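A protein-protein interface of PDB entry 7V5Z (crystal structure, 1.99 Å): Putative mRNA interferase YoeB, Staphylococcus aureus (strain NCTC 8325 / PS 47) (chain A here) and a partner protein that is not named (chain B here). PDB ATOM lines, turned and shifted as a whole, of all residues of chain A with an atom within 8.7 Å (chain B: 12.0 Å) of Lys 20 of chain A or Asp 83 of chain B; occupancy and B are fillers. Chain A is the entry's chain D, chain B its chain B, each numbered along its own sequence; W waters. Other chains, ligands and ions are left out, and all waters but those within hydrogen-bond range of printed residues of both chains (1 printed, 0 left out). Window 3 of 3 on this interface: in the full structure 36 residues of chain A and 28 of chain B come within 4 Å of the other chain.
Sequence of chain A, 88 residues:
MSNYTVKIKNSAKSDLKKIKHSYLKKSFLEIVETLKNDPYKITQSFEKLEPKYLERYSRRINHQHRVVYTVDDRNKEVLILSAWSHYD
Water W1 lies within hydrogen-bond range of the chain-end carboxylate (O) of Leu 85 of chain B (2.5 Å), the side-chain amino group (NZ) of Lys 20 of chain A (3.0 Å) and the backbone carbonyl oxygen (O) of Asp 83 of chain B (3.4 Å).
Hydrophobic or aromatic side chains of chain A within 4 Å of the printed part of chain B: Leu 16 and Phe 28. Among the printed residues, 10 pairs touch across the chains.
OD1 of Asp 81 of chain B lies close to N of Asp 83 of chain B (3.4 Å). O of Lys 17 of chain A sits close to ND1 of His 21 of chain A.
The side-chain amino group of Lys 20 of chain A lies within hydrogen-bond range of the backbone carbonyl oxygen of Trp 82 of chain B (2.7 Å). O of Asp 83 of chain B sits at hydrogen-bond distance from NZ of Lys 20 of chain A.
Printed residues of chain B within 4 Å of Lys 13 of chain A: Ile 80 (3.6 Å). Of the printed residues of chain B, Lys 17 of chain A touches Leu 85 (3.8 Å). No residue of chain B comes within 4 Å of Ile 19 of chain A. Of chain B, only Trp 82 and Asp 83 come within 4 Å of Lys 20 of chain A. No residue of chain B comes within 4 Å of His 21 of chain A. Lys 25 of chain A touches just one residue of chain B: Trp 82. Printed residues of chain A within 4 Å of Ile 80 of chain B: Lys 13 (3.6 Å) and Leu 16 (3.99 Å). Of the printed residues of chain A, Trp 82 of chain B touches Leu 16, Lys 20, Lys 25 and Phe 28. Printed residues of chain A within 4 Å of Leu 85 of chain B: Leu 16 (3.6 Å) and Lys 17 (3.8 Å). The nearest residue of chain B that does not touch Lys 20 of chain A is Asn 84 of chain B (4.2 Å).
Among the printed residues, pairs that only touch across the chains: Lys 13 of chain A with Ile 80 of chain B (3.6 Å), Leu 16 of chain A with Ile 80 of chain B (3.99 Å), Leu 16 of chain A with Trp 82 of chain B (3.7 Å), Leu 16 of chain A with Leu 85 of chain B (3.6 Å), Lys 17 of chain A with Leu 85 of chain B (3.8 Å), Lys 25 of chain A with Trp 82 of chain B (3.5 Å), Phe 28 of chain A with Ile 77 of chain B (3.9 Å) and Phe 28 of chain A with Trp 82 of chain B (3.7 Å).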
ATOM      1  N   LYS A  13      20.127 -10.962  20.862  1.00  0.00           N
ATOM      2  CA  LYS A  13      19.526 -12.198  21.362  1.00  0.00           C
ATOM      3  C   LYS A  13      18.714 -12.917  20.284  1.00  0.00           C
ATOM      4  O   LYS A  13      18.695 -14.150  20.260  1.00  0.00           O
ATOM      5  CB  LYS A  13      18.683 -11.902  22.609  1.00  0.00           C
ATOM      6  CG  LYS A  13      19.558 -11.504  23.804  1.00  0.00           C
ATOM      7  CD  LYS A  13      18.847 -11.661  25.138  1.00  0.00           C
ATOM      8  CE  LYS A  13      18.110 -10.394  25.522  1.00  0.00           C
ATOM      9  NZ  LYS A  13      17.504 -10.480  26.896  1.00  0.00           N
ATOM     10  N   SER A  14      18.080 -12.183  19.352  1.00  0.00           N
ATOM     11  CA  SER A  14      17.399 -12.871  18.251  1.00  0.00           C
ATOM     12  C   SER A  14      18.353 -13.779  17.477  1.00  0.00           C
ATOM     13  O   SER A  14      17.930 -14.825  16.968  1.00  0.00           O
ATOM     14  CB  SER A  14      16.734 -11.872  17.298  1.00  0.00           C
ATOM     15  OG  SER A  14      17.640 -10.872  16.859  1.00  0.00           O
ATOM     16  N   ASP A  15      19.641 -13.405  17.387  1.00  0.00           N
ATOM     17  CA  ASP A  15      20.643 -14.286  16.793  1.00  0.00           C
ATOM     18  C   ASP A  15      20.701 -15.625  17.514  1.00  0.00           C
ATOM     19  O   ASP A  15      20.835 -16.676  16.874  1.00  0.00           O
ATOM     20  CB  ASP A  15      22.036 -13.644  16.833  1.00  0.00           C
ATOM     21  CG  ASP A  15      22.221 -12.534  15.816  1.00  0.00           C
ATOM     22  OD1 ASP A  15      21.261 -12.185  15.094  1.00  0.00           O
ATOM     23  OD2 ASP A  15      23.349 -11.995  15.744  1.00  0.00           O
ATOM     24  N   LEU A  16      20.664 -15.599  18.854  1.00  0.00           N
ATOM     25  CA  LEU A  16      20.770 -16.828  19.627  1.00  0.00           C
ATOM     26  C   LEU A  16      19.561 -17.728  19.419  1.00  0.00           C
ATOM     27  O   LEU A  16      19.693 -18.953  19.473  1.00  0.00           O
ATOM     28  CB  LEU A  16      20.933 -16.513  21.117  1.00  0.00           C
ATOM     29  CG  LEU A  16      22.162 -15.728  21.550  1.00  0.00           C
ATOM     30  CD1 LEU A  16      22.183 -15.626  23.073  1.00  0.00           C
ATOM     31  CD2 LEU A  16      23.460 -16.357  21.009  1.00  0.00           C
ATOM     32  N   LYS A  17      18.382 -17.142  19.191  1.00  0.00           N
ATOM     33  CA  LYS A  17      17.214 -17.942  18.828  1.00  0.00           C
ATOM     34  C   LYS A  17      17.475 -18.748  17.560  1.00  0.00           C
ATOM     35  O   LYS A  17      17.132 -19.933  17.489  1.00  0.00           O
ATOM     36  CB  LYS A  17      15.990 -17.037  18.647  1.00  0.00           C
ATOM     37  CG  LYS A  17      14.648 -17.767  18.621  1.00  0.00           C
ATOM     38  CD  LYS A  17      13.548 -16.951  17.926  1.00  0.00           C
ATOM     39  CE  LYS A  17      13.345 -15.582  18.571  1.00  0.00           C
ATOM     40  NZ  LYS A  17      11.894 -15.220  18.685  1.00  0.00           N
ATOM     41  N   LYS A  18      18.101 -18.131  16.551  1.00  0.00           N
ATOM     42  CA  LYS A  18      18.412 -18.864  15.329  1.00  0.00           C
ATOM     43  C   LYS A  18      19.487 -19.918  15.574  1.00  0.00           C
ATOM     44  O   LYS A  18      19.408 -21.029  15.038  1.00  0.00           O
ATOM     45  CB  LYS A  18      18.840 -17.892  14.225  1.00  0.00           C
ATOM     46  CG  LYS A  18      17.814 -16.796  13.940  1.00  0.00           C
ATOM     47  CD  LYS A  18      18.276 -15.877  12.819  1.00  0.00           C
ATOM     48  CE  LYS A  18      17.451 -14.606  12.754  1.00  0.00           C
ATOM     49  NZ  LYS A  18      18.055 -13.660  11.757  1.00  0.00           N
ATOM     50  N   ILE A  19      20.490 -19.589  16.389  1.00  0.00           N
ATOM     51  CA  ILE A  19      21.514 -20.564  16.761  1.00  0.00           C
ATOM     52  C   ILE A  19      20.873 -21.779  17.431  1.00  0.00           C
ATOM     53  O   ILE A  19      21.196 -22.934  17.117  1.00  0.00           O
ATOM     54  CB  ILE A  19      22.554 -19.897  17.681  1.00  0.00           C
ATOM     55  CG1 ILE A  19      23.427 -18.897  16.896  1.00  0.00           C
ATOM     56  CG2 ILE A  19      23.356 -20.949  18.459  1.00  0.00           C
ATOM     57  CD1 ILE A  19      24.366 -19.537  15.875  1.00  0.00           C
ATOM     58  N   LYS A  20      19.958 -21.530  18.376  1.00  0.00           N
ATOM     59  CA  LYS A  20      19.282 -22.625  19.074  1.00  0.00           C
ATOM     60  C   LYS A  20      18.525 -23.528  18.099  1.00  0.00           C
ATOM     61  O   LYS A  20      18.672 -24.755  18.139  1.00  0.00           O
ATOM     62  CB  LYS A  20      18.332 -22.065  20.135  1.00  0.00           C
ATOM     63  CG  LYS A  20      17.547 -23.161  20.856  1.00  0.00           C
ATOM     64  CD  LYS A  20      16.515 -22.584  21.806  1.00  0.00           C
ATOM     65  CE  LYS A  20      15.768 -23.703  22.525  1.00  0.00           C
ATOM     66  NZ  LYS A  20      15.007 -23.174  23.683  1.00  0.00           N
ATOM     67  N   HIS A  21      17.722 -22.931  17.206  1.00  0.00           N
ATOM     68  CA  HIS A  21      16.952 -23.712  16.231  1.00  0.00           C
ATOM     69  C   HIS A  21      17.849 -24.484  15.272  1.00  0.00           C
ATOM     70  O   HIS A  21      17.469 -25.560  14.797  1.00  0.00           O
ATOM     71  CB  HIS A  21      16.027 -22.798  15.422  1.00  0.00           C
ATOM     72  CG  HIS A  21      14.940 -22.158  16.228  1.00  0.00           C
ATOM     73  ND1 HIS A  21      14.765 -22.399  17.575  1.00  0.00           N
ATOM     74  CD2 HIS A  21      13.976 -21.275  15.877  1.00  0.00           C
ATOM     75  CE1 HIS A  21      13.745 -21.687  18.020  1.00  0.00           C
ATOM     76  NE2 HIS A  21      13.245 -20.999  17.009  1.00  0.00           N
ATOM     77  N   SER A  22      19.024 -23.946  14.961  1.00  0.00           N
ATOM     78  CA  SER A  22      19.982 -24.559  14.057  1.00  0.00           C
ATOM     79  C   SER A  22      20.807 -25.653  14.712  1.00  0.00           C
ATOM     80  O   SER A  22      21.650 -26.250  14.038  1.00  0.00           O
ATOM     81  CB  SER A  22      20.927 -23.482  13.524  1.00  0.00           C
ATOM     82  OG  SER A  22      20.231 -22.636  12.627  1.00  0.00           O
ATOM     83  N   TYR A  23      20.599 -25.901  16.009  1.00  0.00           N
ATOM     84  CA  TYR A  23      21.413 -26.820  16.803  1.00  0.00           C
ATOM     85  C   TYR A  23      22.865 -26.364  16.889  1.00  0.00           C
ATOM     86  O   TYR A  23      23.781 -27.187  17.015  1.00  0.00           O
ATOM     87  CB  TYR A  23      21.341 -28.257  16.276  1.00  0.00           C
ATOM     88  CG  TYR A  23      21.713 -29.256  17.346  1.00  0.00           C
ATOM     89  CD1 TYR A  23      21.053 -29.256  18.577  1.00  0.00           C
ATOM     90  CD2 TYR A  23      22.728 -30.195  17.135  1.00  0.00           C
ATOM     91  CE1 TYR A  23      21.390 -30.158  19.575  1.00  0.00           C
ATOM     92  CE2 TYR A  23      23.074 -31.105  18.124  1.00  0.00           C
ATOM     93  CZ  TYR A  23      22.409 -31.079  19.341  1.00  0.00           C
ATOM     94  OH  TYR A  23      22.745 -31.975  20.320  1.00  0.00           O
ATOM     95  N   LEU A  24      23.087 -25.051  16.834  1.00  0.00           N
ATOM     96  CA  LEU A  24      24.427 -24.501  16.914  1.00  0.00           C
ATOM     97  C   LEU A  24      24.783 -24.057  18.321  1.00  0.00           C
ATOM     98  O   LEU A  24      25.839 -23.441  18.517  1.00  0.00           O
ATOM     99  CB  LEU A  24      24.569 -23.344  15.927  1.00  0.00           C
ATOM    100  CG  LEU A  24      24.499 -23.869  14.500  1.00  0.00           C
ATOM    101  CD1 LEU A  24      24.454 -22.742  13.468  1.00  0.00           C
ATOM    102  CD2 LEU A  24      25.694 -24.767  14.260  1.00  0.00           C
ATOM    103  N   LYS A  25      23.925 -24.348  19.305  1.00  0.00           N
ATOM    104  CA  LYS A  25      24.167 -23.868  20.663  1.00  0.00           C
ATOM    105  C   LYS A  25      25.496 -24.368  21.193  1.00  0.00           C
ATOM    106  O   LYS A  25      26.252 -23.606  21.799  1.00  0.00           O
ATOM    107  CB  LYS A  25      23.045 -24.306  21.604  1.00  0.00           C
ATOM    108  CG  LYS A  25      23.268 -23.936  23.062  1.00  0.00           C
ATOM    109  CD  LYS A  25      22.093 -24.421  23.903  1.00  0.00           C
ATOM    110  CE  LYS A  25      22.238 -24.045  25.366  1.00  0.00           C
ATOM    111  NZ  LYS A  25      21.077 -24.549  26.151  1.00  0.00           N
ATOM    112  N   LYS A  26      25.809 -25.648  20.967  1.00  0.00           N
ATOM    113  CA  LYS A  26      27.050 -26.165  21.527  1.00  0.00           C
ATOM    114  C   LYS A  26      28.273 -25.526  20.866  1.00  0.00           C
ATOM    115  O   LYS A  26      29.247 -25.202  21.553  1.00  0.00           O
ATOM    116  CB  LYS A  26      27.083 -27.691  21.427  1.00  0.00           C
ATOM    117  CG  LYS A  26      28.358 -28.276  21.980  1.00  0.00           C
ATOM    118  CD  LYS A  26      28.290 -29.792  22.159  1.00  0.00           C
ATOM    119  CE  LYS A  26      29.690 -30.384  22.094  1.00  0.00           C
ATOM    120  NZ  LYS A  26      29.876 -31.569  22.985  1.00  0.00           N
ATOM    121  N   PHE A  28      28.386 -22.540  19.566  1.00  0.00           N
ATOM    122  CA  PHE A  28      28.426 -21.156  20.018  1.00  0.00           C
ATOM    123  C   PHE A  28      29.007 -21.050  21.425  1.00  0.00           C
ATOM    124  O   PHE A  28      29.875 -20.210  21.685  1.00  0.00           O
ATOM    125  CB  PHE A  28      27.033 -20.540  19.978  1.00  0.00           C
ATOM    126  CG  PHE A  28      26.966 -19.213  20.650  1.00  0.00           C
ATOM    127  CD1 PHE A  28      27.487 -18.088  20.029  1.00  0.00           C
ATOM    128  CD2 PHE A  28      26.413 -19.089  21.913  1.00  0.00           C
ATOM    129  CE1 PHE A  28      27.451 -16.862  20.666  1.00  0.00           C
ATOM    130  CE2 PHE A  28      26.363 -17.873  22.547  1.00  0.00           C
ATOM    131  CZ  PHE A  28      26.886 -16.761  21.939  1.00  0.00           C
ATOM    132  N   ALA A  83      25.807 -13.289  16.393  1.00  0.00           N
ATOM    133  CA  ALA A  83      26.074 -14.717  16.428  1.00  0.00           C
ATOM    134  C   ALA A  83      25.389 -15.412  15.266  1.00  0.00           C
ATOM    135  O   ALA A  83      25.239 -16.633  15.290  1.00  0.00           O
ATOM    136  CB  ALA A  83      25.626 -15.331  17.757  1.00  0.00           C
ATOM    137  N   TRP A  84      24.978 -14.648  14.255  1.00  0.00           N
ATOM    138  CA  TRP A  84      24.274 -15.165  13.083  1.00  0.00           C
ATOM    139  C   TRP A  84      24.657 -14.284  11.900  1.00  0.00           C
ATOM    140  O   TRP A  84      24.426 -13.072  11.939  1.00  0.00           O
ATOM    141  CB  TRP A  84      22.756 -15.136  13.312  1.00  0.00           C
ATOM    142  CG  TRP A  84      21.928 -15.828  12.250  1.00  0.00           C
ATOM    143  CD1 TRP A  84      21.201 -15.232  11.249  1.00  0.00           C
ATOM    144  CD2 TRP A  84      21.720 -17.238  12.108  1.00  0.00           C
ATOM    145  NE1 TRP A  84      20.569 -16.186  10.492  1.00  0.00           N
ATOM    146  CE2 TRP A  84      20.863 -17.425  10.999  1.00  0.00           C
ATOM    147  CE3 TRP A  84      22.173 -18.363  12.810  1.00  0.00           C
ATOM    148  CZ2 TRP A  84      20.459 -18.682  10.578  1.00  0.00           C
ATOM    149  CZ3 TRP A  84      21.771 -19.618  12.386  1.00  0.00           C
ATOM    150  CH2 TRP A  84      20.920 -19.765  11.284  1.00  0.00           C
ATOM    151  N   ILE B  77      26.531 -13.396  29.226  1.00  0.00           N
ATOM    152  CA  ILE B  77      26.166 -14.531  28.389  1.00  0.00           C
ATOM    153  C   ILE B  77      25.645 -15.696  29.223  1.00  0.00           C
ATOM    154  O   ILE B  77      24.806 -16.478  28.756  1.00  0.00           O
ATOM    155  CB  ILE B  77      27.369 -14.931  27.513  1.00  0.00           C
ATOM    156  CG1 ILE B  77      26.903 -15.867  26.397  1.00  0.00           C
ATOM    157  CG2 ILE B  77      28.489 -15.534  28.372  1.00  0.00           C
ATOM    158  CD1 ILE B  77      25.969 -15.188  25.386  1.00  0.00           C
ATOM    159  N   ASP B  78      26.103 -15.819  30.473  1.00  0.00           N
ATOM    160  CA  ASP B  78      25.634 -16.893  31.343  1.00  0.00           C
ATOM    161  C   ASP B  78      24.210 -16.669  31.852  1.00  0.00           C
ATOM    162  O   ASP B  78      23.579 -17.622  32.323  1.00  0.00           O
ATOM    163  CB  ASP B  78      26.598 -17.065  32.520  1.00  0.00           C
ATOM    164  CG  ASP B  78      27.983 -17.541  32.082  1.00  0.00           C
ATOM    165  OD1 ASP B  78      28.102 -18.169  31.005  1.00  0.00           O
ATOM    166  OD2 ASP B  78      28.965 -17.284  32.813  1.00  0.00           O
ATOM    167  N   ASP B  79      23.684 -15.453  31.751  1.00  0.00           N
ATOM    168  CA  ASP B  79      22.341 -15.140  32.214  1.00  0.00           C
ATOM    169  C   ASP B  79      21.281 -15.308  31.131  1.00  0.00           C
ATOM    170  O   ASP B  79      20.104 -15.063  31.404  1.00  0.00           O
ATOM    171  CB  ASP B  79      22.290 -13.710  32.756  1.00  0.00           C
ATOM    172  CG  ASP B  79      23.179 -13.516  33.981  1.00  0.00           C
ATOM    173  OD1 ASP B  79      23.450 -14.509  34.695  1.00  0.00           O
ATOM    174  OD2 ASP B  79      23.606 -12.368  34.229  1.00  0.00           O
ATOM    175  N   ILE B  80      21.680 -15.678  29.909  1.00  0.00           N
ATOM    176  CA  ILE B  80      20.725 -15.993  28.857  1.00  0.00           C
ATOM    177  C   ILE B  80      19.876 -17.183  29.277  1.00  0.00           C
ATOM    178  O   ILE B  80      20.405 -18.216  29.702  1.00  0.00           O
ATOM    179  CB  ILE B  80      21.463 -16.302  27.547  1.00  0.00           C
ATOM    180  CG1 ILE B  80      22.200 -15.066  27.024  1.00  0.00           C
ATOM    181  CG2 ILE B  80      20.495 -16.869  26.512  1.00  0.00           C
ATOM    182  CD1 ILE B  80      21.270 -13.930  26.604  1.00  0.00           C
ATOM    183  N   ASP B  81      18.556 -17.055  29.131  1.00  0.00           N
ATOM    184  CA  ASP B  81      17.636 -18.180  29.346  1.00  0.00           C
ATOM    185  C   ASP B  81      17.419 -18.879  28.006  1.00  0.00           C
ATOM    186  O   ASP B  81      16.526 -18.520  27.232  1.00  0.00           O
ATOM    187  CB  ASP B  81      16.319 -17.693  29.946  1.00  0.00           C
ATOM    188  CG  ASP B  81      15.321 -18.839  30.206  1.00  0.00           C
ATOM    189  OD1 ASP B  81      15.695 -20.025  30.064  1.00  0.00           O
ATOM    190  OD2 ASP B  81      14.159 -18.547  30.560  1.00  0.00           O
ATOM    191  N   TRP B  82      18.242 -19.899  27.731  1.00  0.00           N
ATOM    192  CA  TRP B  82      18.186 -20.563  26.427  1.00  0.00           C
ATOM    193  C   TRP B  82      16.863 -21.291  26.224  1.00  0.00           C
ATOM    194  O   TRP B  82      16.318 -21.310  25.111  1.00  0.00           O
ATOM    195  CB  TRP B  82      19.339 -21.555  26.274  1.00  0.00           C
ATOM    196  CG  TRP B  82      20.647 -20.920  25.945  1.00  0.00           C
ATOM    197  CD1 TRP B  82      21.587 -20.478  26.830  1.00  0.00           C
ATOM    198  CD2 TRP B  82      21.175 -20.665  24.635  1.00  0.00           C
ATOM    199  NE1 TRP B  82      22.666 -19.956  26.152  1.00  0.00           N
ATOM    200  CE2 TRP B  82      22.435 -20.059  24.804  1.00  0.00           C
ATOM    201  CE3 TRP B  82      20.700 -20.885  23.338  1.00  0.00           C
ATOM    202  CZ2 TRP B  82      23.223 -19.664  23.724  1.00  0.00           C
ATOM    203  CZ3 TRP B  82      21.478 -20.490  22.266  1.00  0.00           C
ATOM    204  CH2 TRP B  82      22.730 -19.891  22.467  1.00  0.00           C
ATOM    205  N   ASP B  83      16.336 -21.901  27.290  1.00  0.00           N
ATOM    206  CA  ASP B  83      15.151 -22.740  27.152  1.00  0.00           C
ATOM    207  C   ASP B  83      13.932 -21.953  26.680  1.00  0.00           C
ATOM    208  O   ASP B  83      13.022 -22.554  26.096  1.00  0.00           O
ATOM    209  CB  ASP B  83      14.832 -23.447  28.479  1.00  0.00           C
ATOM    210  CG  ASP B  83      15.958 -24.375  28.952  1.00  0.00           C
ATOM    211  OD1 ASP B  83      16.769 -24.845  28.120  1.00  0.00           O
ATOM    212  OD2 ASP B  83      16.022 -24.649  30.168  1.00  0.00           O
ATOM    213  N   ASN B  84      13.898 -20.632  26.901  1.00  0.00           N
ATOM    214  CA  ASN B  84      12.743 -19.806  26.551  1.00  0.00           C
ATOM    215  C   ASN B  84      13.046 -18.787  25.458  1.00  0.00           C
ATOM    216  O   ASN B  84      12.288 -17.822  25.290  1.00  0.00           O
ATOM    217  CB  ASN B  84      12.199 -19.075  27.778  1.00  0.00           C
ATOM    218  CG  ASN B  84      11.509 -20.003  28.759  1.00  0.00           C
ATOM    219  OD1 ASN B  84      10.730 -20.882  28.373  1.00  0.00           O
ATOM    220  ND2 ASN B  84      11.794 -19.808  30.048  1.00  0.00           N
ATOM    221  N   LEU B  85      14.134 -18.974  24.720  1.00  0.00           N
ATOM    222  CA  LEU B  85      14.562 -18.009  23.707  1.00  0.00           C
ATOM    223  C   LEU B  85      13.517 -17.846  22.598  1.00  0.00           C
ATOM    224  O   LEU B  85      13.008 -18.839  22.056  1.00  0.00           O
ATOM    225  CB  LEU B  85      15.900 -18.456  23.125  1.00  0.00           C
ATOM    226  CG  LEU B  85      17.030 -17.465  22.896  1.00  0.00           C
ATOM    227  CD1 LEU B  85      17.082 -16.399  23.968  1.00  0.00           C
ATOM    228  CD2 LEU B  85      18.314 -18.262  22.884  1.00  0.00           C
ATOM    229  OXT LEU B  85      13.152 -16.720  22.230  1.00  0.00           O
HETATM  230  O   HOH W   1      12.935 -21.210  22.930  1.00  0.00           O
